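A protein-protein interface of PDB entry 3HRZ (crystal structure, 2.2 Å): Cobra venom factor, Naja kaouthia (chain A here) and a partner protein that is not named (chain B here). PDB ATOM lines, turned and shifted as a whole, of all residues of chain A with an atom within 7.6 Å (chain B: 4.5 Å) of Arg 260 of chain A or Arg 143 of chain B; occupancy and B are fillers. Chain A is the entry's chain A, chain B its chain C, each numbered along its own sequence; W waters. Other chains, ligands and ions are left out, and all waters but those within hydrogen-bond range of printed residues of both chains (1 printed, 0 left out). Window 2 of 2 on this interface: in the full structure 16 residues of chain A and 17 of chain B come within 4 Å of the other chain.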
ATOM      1  N   VAL A 238      13.350 -27.141  -4.059  1.00  0.00           N
ATOM      2  CA  VAL A 238      14.468 -27.361  -3.148  1.00  0.00           C
ATOM      3  C   VAL A 238      13.902 -27.573  -1.741  1.00  0.00           C
ATOM      4  O   VAL A 238      12.847 -27.028  -1.409  1.00  0.00           O
ATOM      5  CB  VAL A 238      15.440 -26.145  -3.181  1.00  0.00           C
ATOM      6  CG1 VAL A 238      16.469 -26.237  -2.087  1.00  0.00           C
ATOM      7  CG2 VAL A 238      16.142 -26.042  -4.555  1.00  0.00           C
ATOM      8  N   ALA A 239      14.589 -28.378  -0.933  1.00  0.00           N
ATOM      9  CA  ALA A 239      14.203 -28.602   0.449  1.00  0.00           C
ATOM     10  C   ALA A 239      15.385 -28.364   1.393  1.00  0.00           C
ATOM     11  O   ALA A 239      16.534 -28.692   1.079  1.00  0.00           O
ATOM     12  CB  ALA A 239      13.645 -30.023   0.635  1.00  0.00           C
ATOM     13  N   PHE A 240      15.090 -27.769   2.543  1.00  0.00           N
ATOM     14  CA  PHE A 240      16.082 -27.550   3.587  1.00  0.00           C
ATOM     15  C   PHE A 240      15.647 -28.381   4.801  1.00  0.00           C
ATOM     16  O   PHE A 240      14.561 -28.171   5.372  1.00  0.00           O
ATOM     17  CB  PHE A 240      16.164 -26.070   3.958  1.00  0.00           C
ATOM     18  CG  PHE A 240      16.682 -25.192   2.854  1.00  0.00           C
ATOM     19  CD1 PHE A 240      18.042 -24.964   2.710  1.00  0.00           C
ATOM     20  CD2 PHE A 240      15.812 -24.603   1.953  1.00  0.00           C
ATOM     21  CE1 PHE A 240      18.528 -24.149   1.679  1.00  0.00           C
ATOM     22  CE2 PHE A 240      16.284 -23.787   0.927  1.00  0.00           C
ATOM     23  CZ  PHE A 240      17.647 -23.562   0.791  1.00  0.00           C
ATOM     24  N   VAL A 241      16.494 -29.325   5.190  1.00  0.00           N
ATOM     25  CA  VAL A 241      16.150 -30.257   6.250  1.00  0.00           C
ATOM     26  C   VAL A 241      17.088 -30.090   7.432  1.00  0.00           C
ATOM     27  O   VAL A 241      18.300 -30.058   7.275  1.00  0.00           O
ATOM     28  CB  VAL A 241      16.236 -31.688   5.745  1.00  0.00           C
ATOM     29  CG1 VAL A 241      15.947 -32.681   6.899  1.00  0.00           C
ATOM     30  CG2 VAL A 241      15.268 -31.865   4.593  1.00  0.00           C
ATOM     31  N   LEU A 242      16.513 -29.956   8.615  1.00  0.00           N
ATOM     32  CA  LEU A 242      17.296 -29.811   9.822  1.00  0.00           C
ATOM     33  C   LEU A 242      16.811 -30.865  10.806  1.00  0.00           C
ATOM     34  O   LEU A 242      15.613 -30.917  11.119  1.00  0.00           O
ATOM     35  CB  LEU A 242      17.086 -28.420  10.429  1.00  0.00           C
ATOM     36  CG  LEU A 242      17.794 -28.170  11.764  1.00  0.00           C
ATOM     37  CD1 LEU A 242      19.347 -28.147  11.594  1.00  0.00           C
ATOM     38  CD2 LEU A 242      17.294 -26.879  12.389  1.00  0.00           C
ATOM     39  N   SER A 257      23.651 -30.807  10.839  1.00  0.00           N
ATOM     40  CA  SER A 257      22.799 -31.663  10.020  1.00  0.00           C
ATOM     41  C   SER A 257      21.987 -30.883   8.987  1.00  0.00           C
ATOM     42  O   SER A 257      21.366 -31.487   8.117  1.00  0.00           O
ATOM     43  CB  SER A 257      21.829 -32.478  10.883  1.00  0.00           C
ATOM     44  OG  SER A 257      20.711 -31.688  11.258  1.00  0.00           O
ATOM     45  N   LEU A 258      21.968 -29.559   9.087  1.00  0.00           N
ATOM     46  CA  LEU A 258      21.208 -28.744   8.133  1.00  0.00           C
ATOM     47  C   LEU A 258      21.660 -29.066   6.716  1.00  0.00           C
ATOM     48  O   LEU A 258      22.834 -28.940   6.384  1.00  0.00           O
ATOM     49  CB  LEU A 258      21.391 -27.242   8.407  1.00  0.00           C
ATOM     50  CG  LEU A 258      20.683 -26.281   7.427  1.00  0.00           C
ATOM     51  CD1 LEU A 258      19.177 -26.560   7.379  1.00  0.00           C
ATOM     52  CD2 LEU A 258      20.948 -24.798   7.786  1.00  0.00           C
ATOM     53  N   THR A 259      20.724 -29.477   5.875  1.00  0.00           N
ATOM     54  CA  THR A 259      21.080 -29.906   4.536  1.00  0.00           C
ATOM     55  C   THR A 259      20.091 -29.362   3.492  1.00  0.00           C
ATOM     56  O   THR A 259      18.895 -29.243   3.752  1.00  0.00           O
ATOM     57  CB  THR A 259      21.168 -31.465   4.475  1.00  0.00           C
ATOM     58  OG1 THR A 259      21.459 -31.892   3.146  1.00  0.00           O
ATOM     59  CG2 THR A 259      19.854 -32.088   4.918  1.00  0.00           C
ATOM     60  N   ARG A 260      20.607 -29.053   2.312  1.00  0.00           N
ATOM     61  CA  ARG A 260      19.801 -28.522   1.230  1.00  0.00           C
ATOM     62  C   ARG A 260      19.768 -29.563   0.121  1.00  0.00           C
ATOM     63  O   ARG A 260      20.801 -29.980  -0.375  1.00  0.00           O
ATOM     64  CB  ARG A 260      20.416 -27.215   0.686  1.00  0.00           C
ATOM     65  CG  ARG A 260      19.601 -26.603  -0.454  1.00  0.00           C
ATOM     66  CD  ARG A 260      20.336 -25.460  -1.166  1.00  0.00           C
ATOM     67  NE  ARG A 260      21.651 -25.878  -1.654  1.00  0.00           N
ATOM     68  CZ  ARG A 260      22.788 -25.245  -1.378  1.00  0.00           C
ATOM     69  NH1 ARG A 260      22.780 -24.137  -0.640  1.00  0.00           N
ATOM     70  NH2 ARG A 260      23.933 -25.713  -1.850  1.00  0.00           N
ATOM     71  N   ILE A 261      18.581 -29.967  -0.292  1.00  0.00           N
ATOM     72  CA  ILE A 261      18.501 -31.009  -1.289  1.00  0.00           C
ATOM     73  C   ILE A 261      17.481 -30.683  -2.356  1.00  0.00           C
ATOM     74  O   ILE A 261      16.456 -30.082  -2.080  1.00  0.00           O
ATOM     75  CB  ILE A 261      18.131 -32.363  -0.650  1.00  0.00           C
ATOM     76  CG1 ILE A 261      16.796 -32.242   0.050  1.00  0.00           C
ATOM     77  CG2 ILE A 261      19.219 -32.821   0.343  1.00  0.00           C
ATOM     78  CD1 ILE A 261      16.246 -33.568   0.489  1.00  0.00           C
ATOM     79  N   PRO A 262      17.762 -31.107  -3.587  1.00  0.00           N
ATOM     80  CA  PRO A 262      16.884 -30.838  -4.730  1.00  0.00           C
ATOM     81  C   PRO A 262      15.583 -31.624  -4.634  1.00  0.00           C
ATOM     82  O   PRO A 262      15.586 -32.770  -4.209  1.00  0.00           O
ATOM     83  CB  PRO A 262      17.689 -31.341  -5.935  1.00  0.00           C
ATOM     84  CG  PRO A 262      19.068 -31.682  -5.412  1.00  0.00           C
ATOM     85  CD  PRO A 262      18.958 -31.891  -3.943  1.00  0.00           C
ATOM     86  N   ILE A 263      14.477 -31.007  -5.029  1.00  0.00           N
ATOM     87  CA  ILE A 263      13.235 -31.736  -5.161  1.00  0.00           C
ATOM     88  C   ILE A 263      12.933 -31.847  -6.650  1.00  0.00           C
ATOM     89  O   ILE A 263      12.511 -30.880  -7.292  1.00  0.00           O
ATOM     90  CB  ILE A 263      12.088 -31.055  -4.393  1.00  0.00           C
ATOM     91  CG1 ILE A 263      12.420 -31.023  -2.910  1.00  0.00           C
ATOM     92  CG2 ILE A 263      10.789 -31.826  -4.573  1.00  0.00           C
ATOM     93  CD1 ILE A 263      12.532 -32.402  -2.303  1.00  0.00           C
ATOM     94  N   LYS A 269      15.441 -36.907  -0.912  1.00  0.00           N
ATOM     95  CA  LYS A 269      15.811 -37.703   0.247  1.00  0.00           C
ATOM     96  C   LYS A 269      16.829 -36.914   1.059  1.00  0.00           C
ATOM     97  O   LYS A 269      17.816 -36.446   0.511  1.00  0.00           O
ATOM     98  CB  LYS A 269      16.394 -39.042  -0.207  1.00  0.00           C
ATOM     99  CG  LYS A 269      16.801 -39.981   0.923  1.00  0.00           C
ATOM    100  CD  LYS A 269      17.379 -41.305   0.372  1.00  0.00           C
ATOM    101  CE  LYS A 269      18.655 -41.711   1.104  1.00  0.00           C
ATOM    102  NZ  LYS A 269      19.269 -42.994   0.602  1.00  0.00           N
ATOM    103  N   ALA A 270      16.558 -36.728   2.349  1.00  0.00           N
ATOM    104  CA  ALA A 270      17.504 -36.077   3.252  1.00  0.00           C
ATOM    105  C   ALA A 270      18.049 -37.099   4.238  1.00  0.00           C
ATOM    106  O   ALA A 270      17.334 -38.014   4.667  1.00  0.00           O
ATOM    107  CB  ALA A 270      16.834 -34.919   4.008  1.00  0.00           C
ATOM    108  N   MET B 116      23.081 -20.917   4.554  1.00  0.00           N
ATOM    109  CA  MET B 116      22.001 -21.203   3.628  1.00  0.00           C
ATOM    110  C   MET B 116      21.234 -19.919   3.267  1.00  0.00           C
ATOM    111  O   MET B 116      20.087 -19.716   3.668  1.00  0.00           O
ATOM    112  CB  MET B 116      21.064 -22.258   4.231  1.00  0.00           C
ATOM    113  CG  MET B 116      21.742 -23.615   4.474  1.00  0.00           C
ATOM    114  SD  MET B 116      22.277 -24.317   2.890  1.00  0.00           S
ATOM    115  CE  MET B 116      22.993 -25.897   3.420  1.00  0.00           C
ATOM    116  N   LEU B 137      27.991 -18.762 -13.213  1.00  0.00           N
ATOM    117  CA  LEU B 137      27.560 -18.495 -11.844  1.00  0.00           C
ATOM    118  C   LEU B 137      27.259 -19.745 -11.019  1.00  0.00           C
ATOM    119  O   LEU B 137      27.450 -19.737  -9.806  1.00  0.00           O
ATOM    120  CB  LEU B 137      26.307 -17.627 -11.846  1.00  0.00           C
ATOM    121  CG  LEU B 137      26.482 -16.122 -11.728  1.00  0.00           C
ATOM    122  CD1 LEU B 137      25.113 -15.476 -11.591  1.00  0.00           C
ATOM    123  CD2 LEU B 137      27.361 -15.807 -10.530  1.00  0.00           C
ATOM    124  N   LYS B 139      28.619 -22.559 -10.908  1.00  0.00           N
ATOM    125  CA  LYS B 139      29.814 -23.313 -10.544  1.00  0.00           C
ATOM    126  C   LYS B 139      30.295 -23.013  -9.127  1.00  0.00           C
ATOM    127  O   LYS B 139      30.102 -21.917  -8.604  1.00  0.00           O
ATOM    128  CB  LYS B 139      30.937 -22.986 -11.522  1.00  0.00           C
ATOM    129  CG  LYS B 139      30.540 -23.112 -12.963  1.00  0.00           C
ATOM    130  CD  LYS B 139      30.379 -24.561 -13.361  1.00  0.00           C
ATOM    131  CE  LYS B 139      30.241 -24.691 -14.875  1.00  0.00           C
ATOM    132  NZ  LYS B 139      31.331 -23.990 -15.624  1.00  0.00           N
ATOM    133  N   GLY B 140      30.950 -23.985  -8.515  1.00  0.00           N
ATOM    134  CA  GLY B 140      31.465 -23.795  -7.174  1.00  0.00           C
ATOM    135  C   GLY B 140      30.860 -24.775  -6.191  1.00  0.00           C
ATOM    136  O   GLY B 140      29.695 -25.166  -6.310  1.00  0.00           O
ATOM    137  N   VAL B 141      31.663 -25.164  -5.208  1.00  0.00           N
ATOM    138  CA  VAL B 141      31.261 -26.129  -4.201  1.00  0.00           C
ATOM    139  C   VAL B 141      30.472 -25.432  -3.081  1.00  0.00           C
ATOM    140  O   VAL B 141      30.235 -26.005  -2.017  1.00  0.00           O
ATOM    141  CB  VAL B 141      32.517 -26.876  -3.662  1.00  0.00           C
ATOM    142  CG1 VAL B 141      32.227 -27.629  -2.377  1.00  0.00           C
ATOM    143  CG2 VAL B 141      33.064 -27.821  -4.727  1.00  0.00           C
ATOM    144  N   ASP B 142      30.041 -24.199  -3.339  1.00  0.00           N
ATOM    145  CA  ASP B 142      29.418 -23.380  -2.298  1.00  0.00           C
ATOM    146  C   ASP B 142      28.067 -22.814  -2.710  1.00  0.00           C
ATOM    147  O   ASP B 142      27.472 -22.016  -1.979  1.00  0.00           O
ATOM    148  CB  ASP B 142      30.343 -22.221  -1.917  1.00  0.00           C
ATOM    149  CG  ASP B 142      30.417 -21.159  -2.999  1.00  0.00           C
ATOM    150  OD1 ASP B 142      30.302 -21.511  -4.196  1.00  0.00           O
ATOM    151  OD2 ASP B 142      30.588 -19.971  -2.651  1.00  0.00           O
ATOM    152  N   ARG B 143      27.591 -23.222  -3.882  1.00  0.00           N
ATOM    153  CA  ARG B 143      26.382 -22.645  -4.467  1.00  0.00           C
ATOM    154  C   ARG B 143      25.491 -23.716  -5.048  1.00  0.00           C
ATOM    155  O   ARG B 143      25.901 -24.868  -5.193  1.00  0.00           O
ATOM    156  CB  ARG B 143      26.747 -21.680  -5.586  1.00  0.00           C
ATOM    157  CG  ARG B 143      27.337 -20.406  -5.093  1.00  0.00           C
ATOM    158  CD  ARG B 143      28.397 -19.897  -6.054  1.00  0.00           C
ATOM    159  NE  ARG B 143      28.783 -18.538  -5.703  1.00  0.00           N
ATOM    160  CZ  ARG B 143      28.226 -17.459  -6.241  1.00  0.00           C
ATOM    161  NH1 ARG B 143      27.283 -17.614  -7.160  1.00  0.00           N
ATOM    162  NH2 ARG B 143      28.611 -16.236  -5.879  1.00  0.00           N
ATOM    163  N   TYR B 144      24.269 -23.325  -5.392  1.00  0.00           N
ATOM    164  CA  TYR B 144      23.380 -24.210  -6.123  1.00  0.00           C
ATOM    165  C   TYR B 144      22.367 -23.384  -6.868  1.00  0.00           C
ATOM    166  O   TYR B 144      21.835 -22.403  -6.346  1.00  0.00           O
ATOM    167  CB  TYR B 144      22.693 -25.237  -5.208  1.00  0.00           C
ATOM    168  CG  TYR B 144      21.726 -26.139  -5.958  1.00  0.00           C
ATOM    169  CD1 TYR B 144      22.189 -27.177  -6.758  1.00  0.00           C
ATOM    170  CD2 TYR B 144      20.350 -25.928  -5.888  1.00  0.00           C
ATOM    171  CE1 TYR B 144      21.307 -27.981  -7.463  1.00  0.00           C
ATOM    172  CE2 TYR B 144      19.462 -26.728  -6.585  1.00  0.00           C
ATOM    173  CZ  TYR B 144      19.942 -27.760  -7.363  1.00  0.00           C
ATOM    174  OH  TYR B 144      19.051 -28.554  -8.056  1.00  0.00           O
ATOM    175  N   ILE B 162      19.195 -18.350  -6.513  1.00  0.00           N
ATOM    176  CA  ILE B 162      20.549 -18.787  -6.282  1.00  0.00           C
ATOM    177  C   ILE B 162      20.661 -19.087  -4.810  1.00  0.00           C
ATOM    178  O   ILE B 162      20.345 -18.235  -3.981  1.00  0.00           O
ATOM    179  CB  ILE B 162      21.557 -17.706  -6.655  1.00  0.00           C
ATOM    180  CG1 ILE B 162      21.330 -17.252  -8.105  1.00  0.00           C
ATOM    181  CG2 ILE B 162      22.973 -18.225  -6.454  1.00  0.00           C
ATOM    182  CD1 ILE B 162      21.904 -15.876  -8.415  1.00  0.00           C
ATOM    183  N   TYR B 163      21.069 -20.317  -4.497  1.00  0.00           N
ATOM    184  CA  TYR B 163      21.225 -20.768  -3.124  1.00  0.00           C
ATOM    185  C   TYR B 163      22.698 -20.741  -2.767  1.00  0.00           C
ATOM    186  O   TYR B 163      23.506 -21.380  -3.432  1.00  0.00           O
ATOM    187  CB  TYR B 163      20.670 -22.193  -2.964  1.00  0.00           C
ATOM    188  CG  TYR B 163      19.245 -22.335  -3.457  1.00  0.00           C
ATOM    189  CD1 TYR B 163      18.171 -22.111  -2.608  1.00  0.00           C
ATOM    190  CD2 TYR B 163      18.976 -22.676  -4.770  1.00  0.00           C
ATOM    191  CE1 TYR B 163      16.882 -22.223  -3.051  1.00  0.00           C
ATOM    192  CE2 TYR B 163      17.685 -22.795  -5.222  1.00  0.00           C
ATOM    193  CZ  TYR B 163      16.642 -22.567  -4.355  1.00  0.00           C
ATOM    194  OH  TYR B 163      15.346 -22.686  -4.791  1.00  0.00           O
ATOM    195  N   LEU B 164      23.039 -19.992  -1.721  1.00  0.00           N
ATOM    196  CA  LEU B 164      24.422 -19.856  -1.260  1.00  0.00           C
ATOM    197  C   LEU B 164      24.632 -20.632   0.046  1.00  0.00           C
ATOM    198  O   LEU B 164      23.768 -20.615   0.918  1.00  0.00           O
ATOM    199  CB  LEU B 164      24.739 -18.375  -1.024  1.00  0.00           C
ATOM    200  CG  LEU B 164      25.305 -17.520  -2.169  1.00  0.00           C
ATOM    201  CD1 LEU B 164      25.036 -18.117  -3.537  1.00  0.00           C
ATOM    202  CD2 LEU B 164      24.774 -16.098  -2.085  1.00  0.00           C
ATOM    203  N   ASN B 165      25.769 -21.303   0.191  1.00  0.00           N
ATOM    204  CA  ASN B 165      26.044 -22.018   1.429  1.00  0.00           C
ATOM    205  C   ASN B 165      26.178 -21.030   2.564  1.00  0.00           C
ATOM    206  O   ASN B 165      25.818 -21.318   3.705  1.00  0.00           O
ATOM    207  CB  ASN B 165      27.285 -22.915   1.317  1.00  0.00           C
ATOM    208  CG  ASN B 165      27.007 -24.176   0.522  1.00  0.00           C
ATOM    209  OD1 ASN B 165      25.882 -24.392   0.070  1.00  0.00           O
ATOM    210  ND2 ASN B 165      28.025 -25.015   0.343  1.00  0.00           N
ATOM    211  N   LEU B 175      27.480 -10.426  -7.300  1.00  0.00           N
ATOM    212  CA  LEU B 175      27.448 -11.236  -8.500  1.00  0.00           C
ATOM    213  C   LEU B 175      26.823 -10.448  -9.629  1.00  0.00           C
ATOM    214  O   LEU B 175      26.204  -9.407  -9.409  1.00  0.00           O
ATOM    215  CB  LEU B 175      26.718 -12.554  -8.263  1.00  0.00           C
ATOM    216  CG  LEU B 175      25.332 -12.485  -7.632  1.00  0.00           C
ATOM    217  CD1 LEU B 175      24.267 -12.298  -8.702  1.00  0.00           C
ATOM    218  CD2 LEU B 175      25.084 -13.762  -6.857  1.00  0.00           C
HETATM  219  O   HOH W   1      20.848 -21.866   0.367  1.00  0.00           O
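The side-chain sulfur (SD) of Met 116 of chain B sits at hydrogen-bond distance from the guanidinium group (NH1) of Arg 260 of chain A. The guanidinium group of Arg 260 of chain A is in hydrogen-bond range of the side-chain amide oxygen of Asn 165 of chain B, at 3.0 Å.
The backbone NH of Met 116 of chain B sits at hydrogen-bond distance from the backbone carbonyl oxygen of Asn 165 of chain B, at 2.9 Å. The backbone carbonyl oxygen (O) of Leu 137 of chain B is in hydrogen-bond range of the guanidinium group (NH1) of Arg 143 of chain B (3.4 Å). O of Val 141 of chain B sits at hydrogen-bond distance from ND2 of Asn 165 of chain B (3.4 Å). OD1 of Asp 142 of chain B lies within salt-bridge range of NE of Arg 143 of chain B, at 3.7 Å. N of Asn 165 of chain B is in hydrogen-bond range of O of Asp 142 of chain B, 2.8 Å away. N of Tyr 144 of chain B lies within hydrogen-bond range of O of Tyr 163 of chain B, 2.9 Å away.
Val 238 of chain A touches Tyr 144 of chain B. OH of Tyr 163 of chain B touches CG2 of Val 238 of chain A, 3.5 Å away. Phe 240 of chain A touches Met 116 of chain B. Tyr 163 of chain B touches Phe 240 of chain A. Leu 258 of chain A touches Met 116 of chain B. Arg 143 of chain B touches Arg 260 of chain A (O to NH2, 3.97 Å). NH2 of Arg 260 of chain A touches CB of Tyr 144 of chain B, 3.6 Å away. Arg 260 of chain A touches Tyr 163 of chain B (NH1 to CB, 3.7 Å). NH1 of Arg 260 of chain A touches O of Leu 164 of chain B, 3.98 Å away. CB of Pro 262 of chain A touches OH of Tyr 144 of chain B, at 3.8 Å.
Printed residues of chain B within 4 Å of Leu 258 of chain A: Met 116. Of chain B, only Met 116 (3.6 Å), Arg 143 (3.97 Å), Tyr 144 (3.6 Å), Tyr 163 (3.7 Å), Leu 164 (3.98 Å) and Asn 165 (3.0 Å) come within 4 Å of Arg 260 of chain A. Printed residues of chain A within 4 Å of Met 116 of chain B: Phe 240 (3.9 Å), Leu 258 (3.6 Å) and Arg 260 (3.6 Å). Of chain A, only Arg 260 comes within 4 Å of Arg 143 of chain B. Of the printed residues of chain A, Tyr 144 of chain B touches Val 238, Arg 260 and Pro 262. The nearest printed residue of chain B that does not touch Arg 260 of chain A is Asp 142 of chain B (5.1 Å).
Of the 13 printed residues of chain B, 6 touch a printed residue of chain A. Printed residues of chain B that touch a printed residue of chain A: Met 116, Arg 143, Tyr 144, Tyr 163, Leu 164 and Asn 165. Hydrophobic or aromatic side chains of chain B that line the printed part of chain A: Met 116, Tyr 144 and Tyr 163. Hydrophobic or aromatic side chains of chain A within 4 Å of the printed part of chain B: Val 238, Phe 240, Leu 258 and Pro 262.
Water W1 lies within hydrogen-bond range of the guanidinium group (NH1) of Arg 260 of chain A (3.1 Å), the backbone carbonyl oxygen (O) of Leu 164 of chain B (3.2 Å) and the side-chain sulfur (SD) of Met 116 of chain B (3.8 Å).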
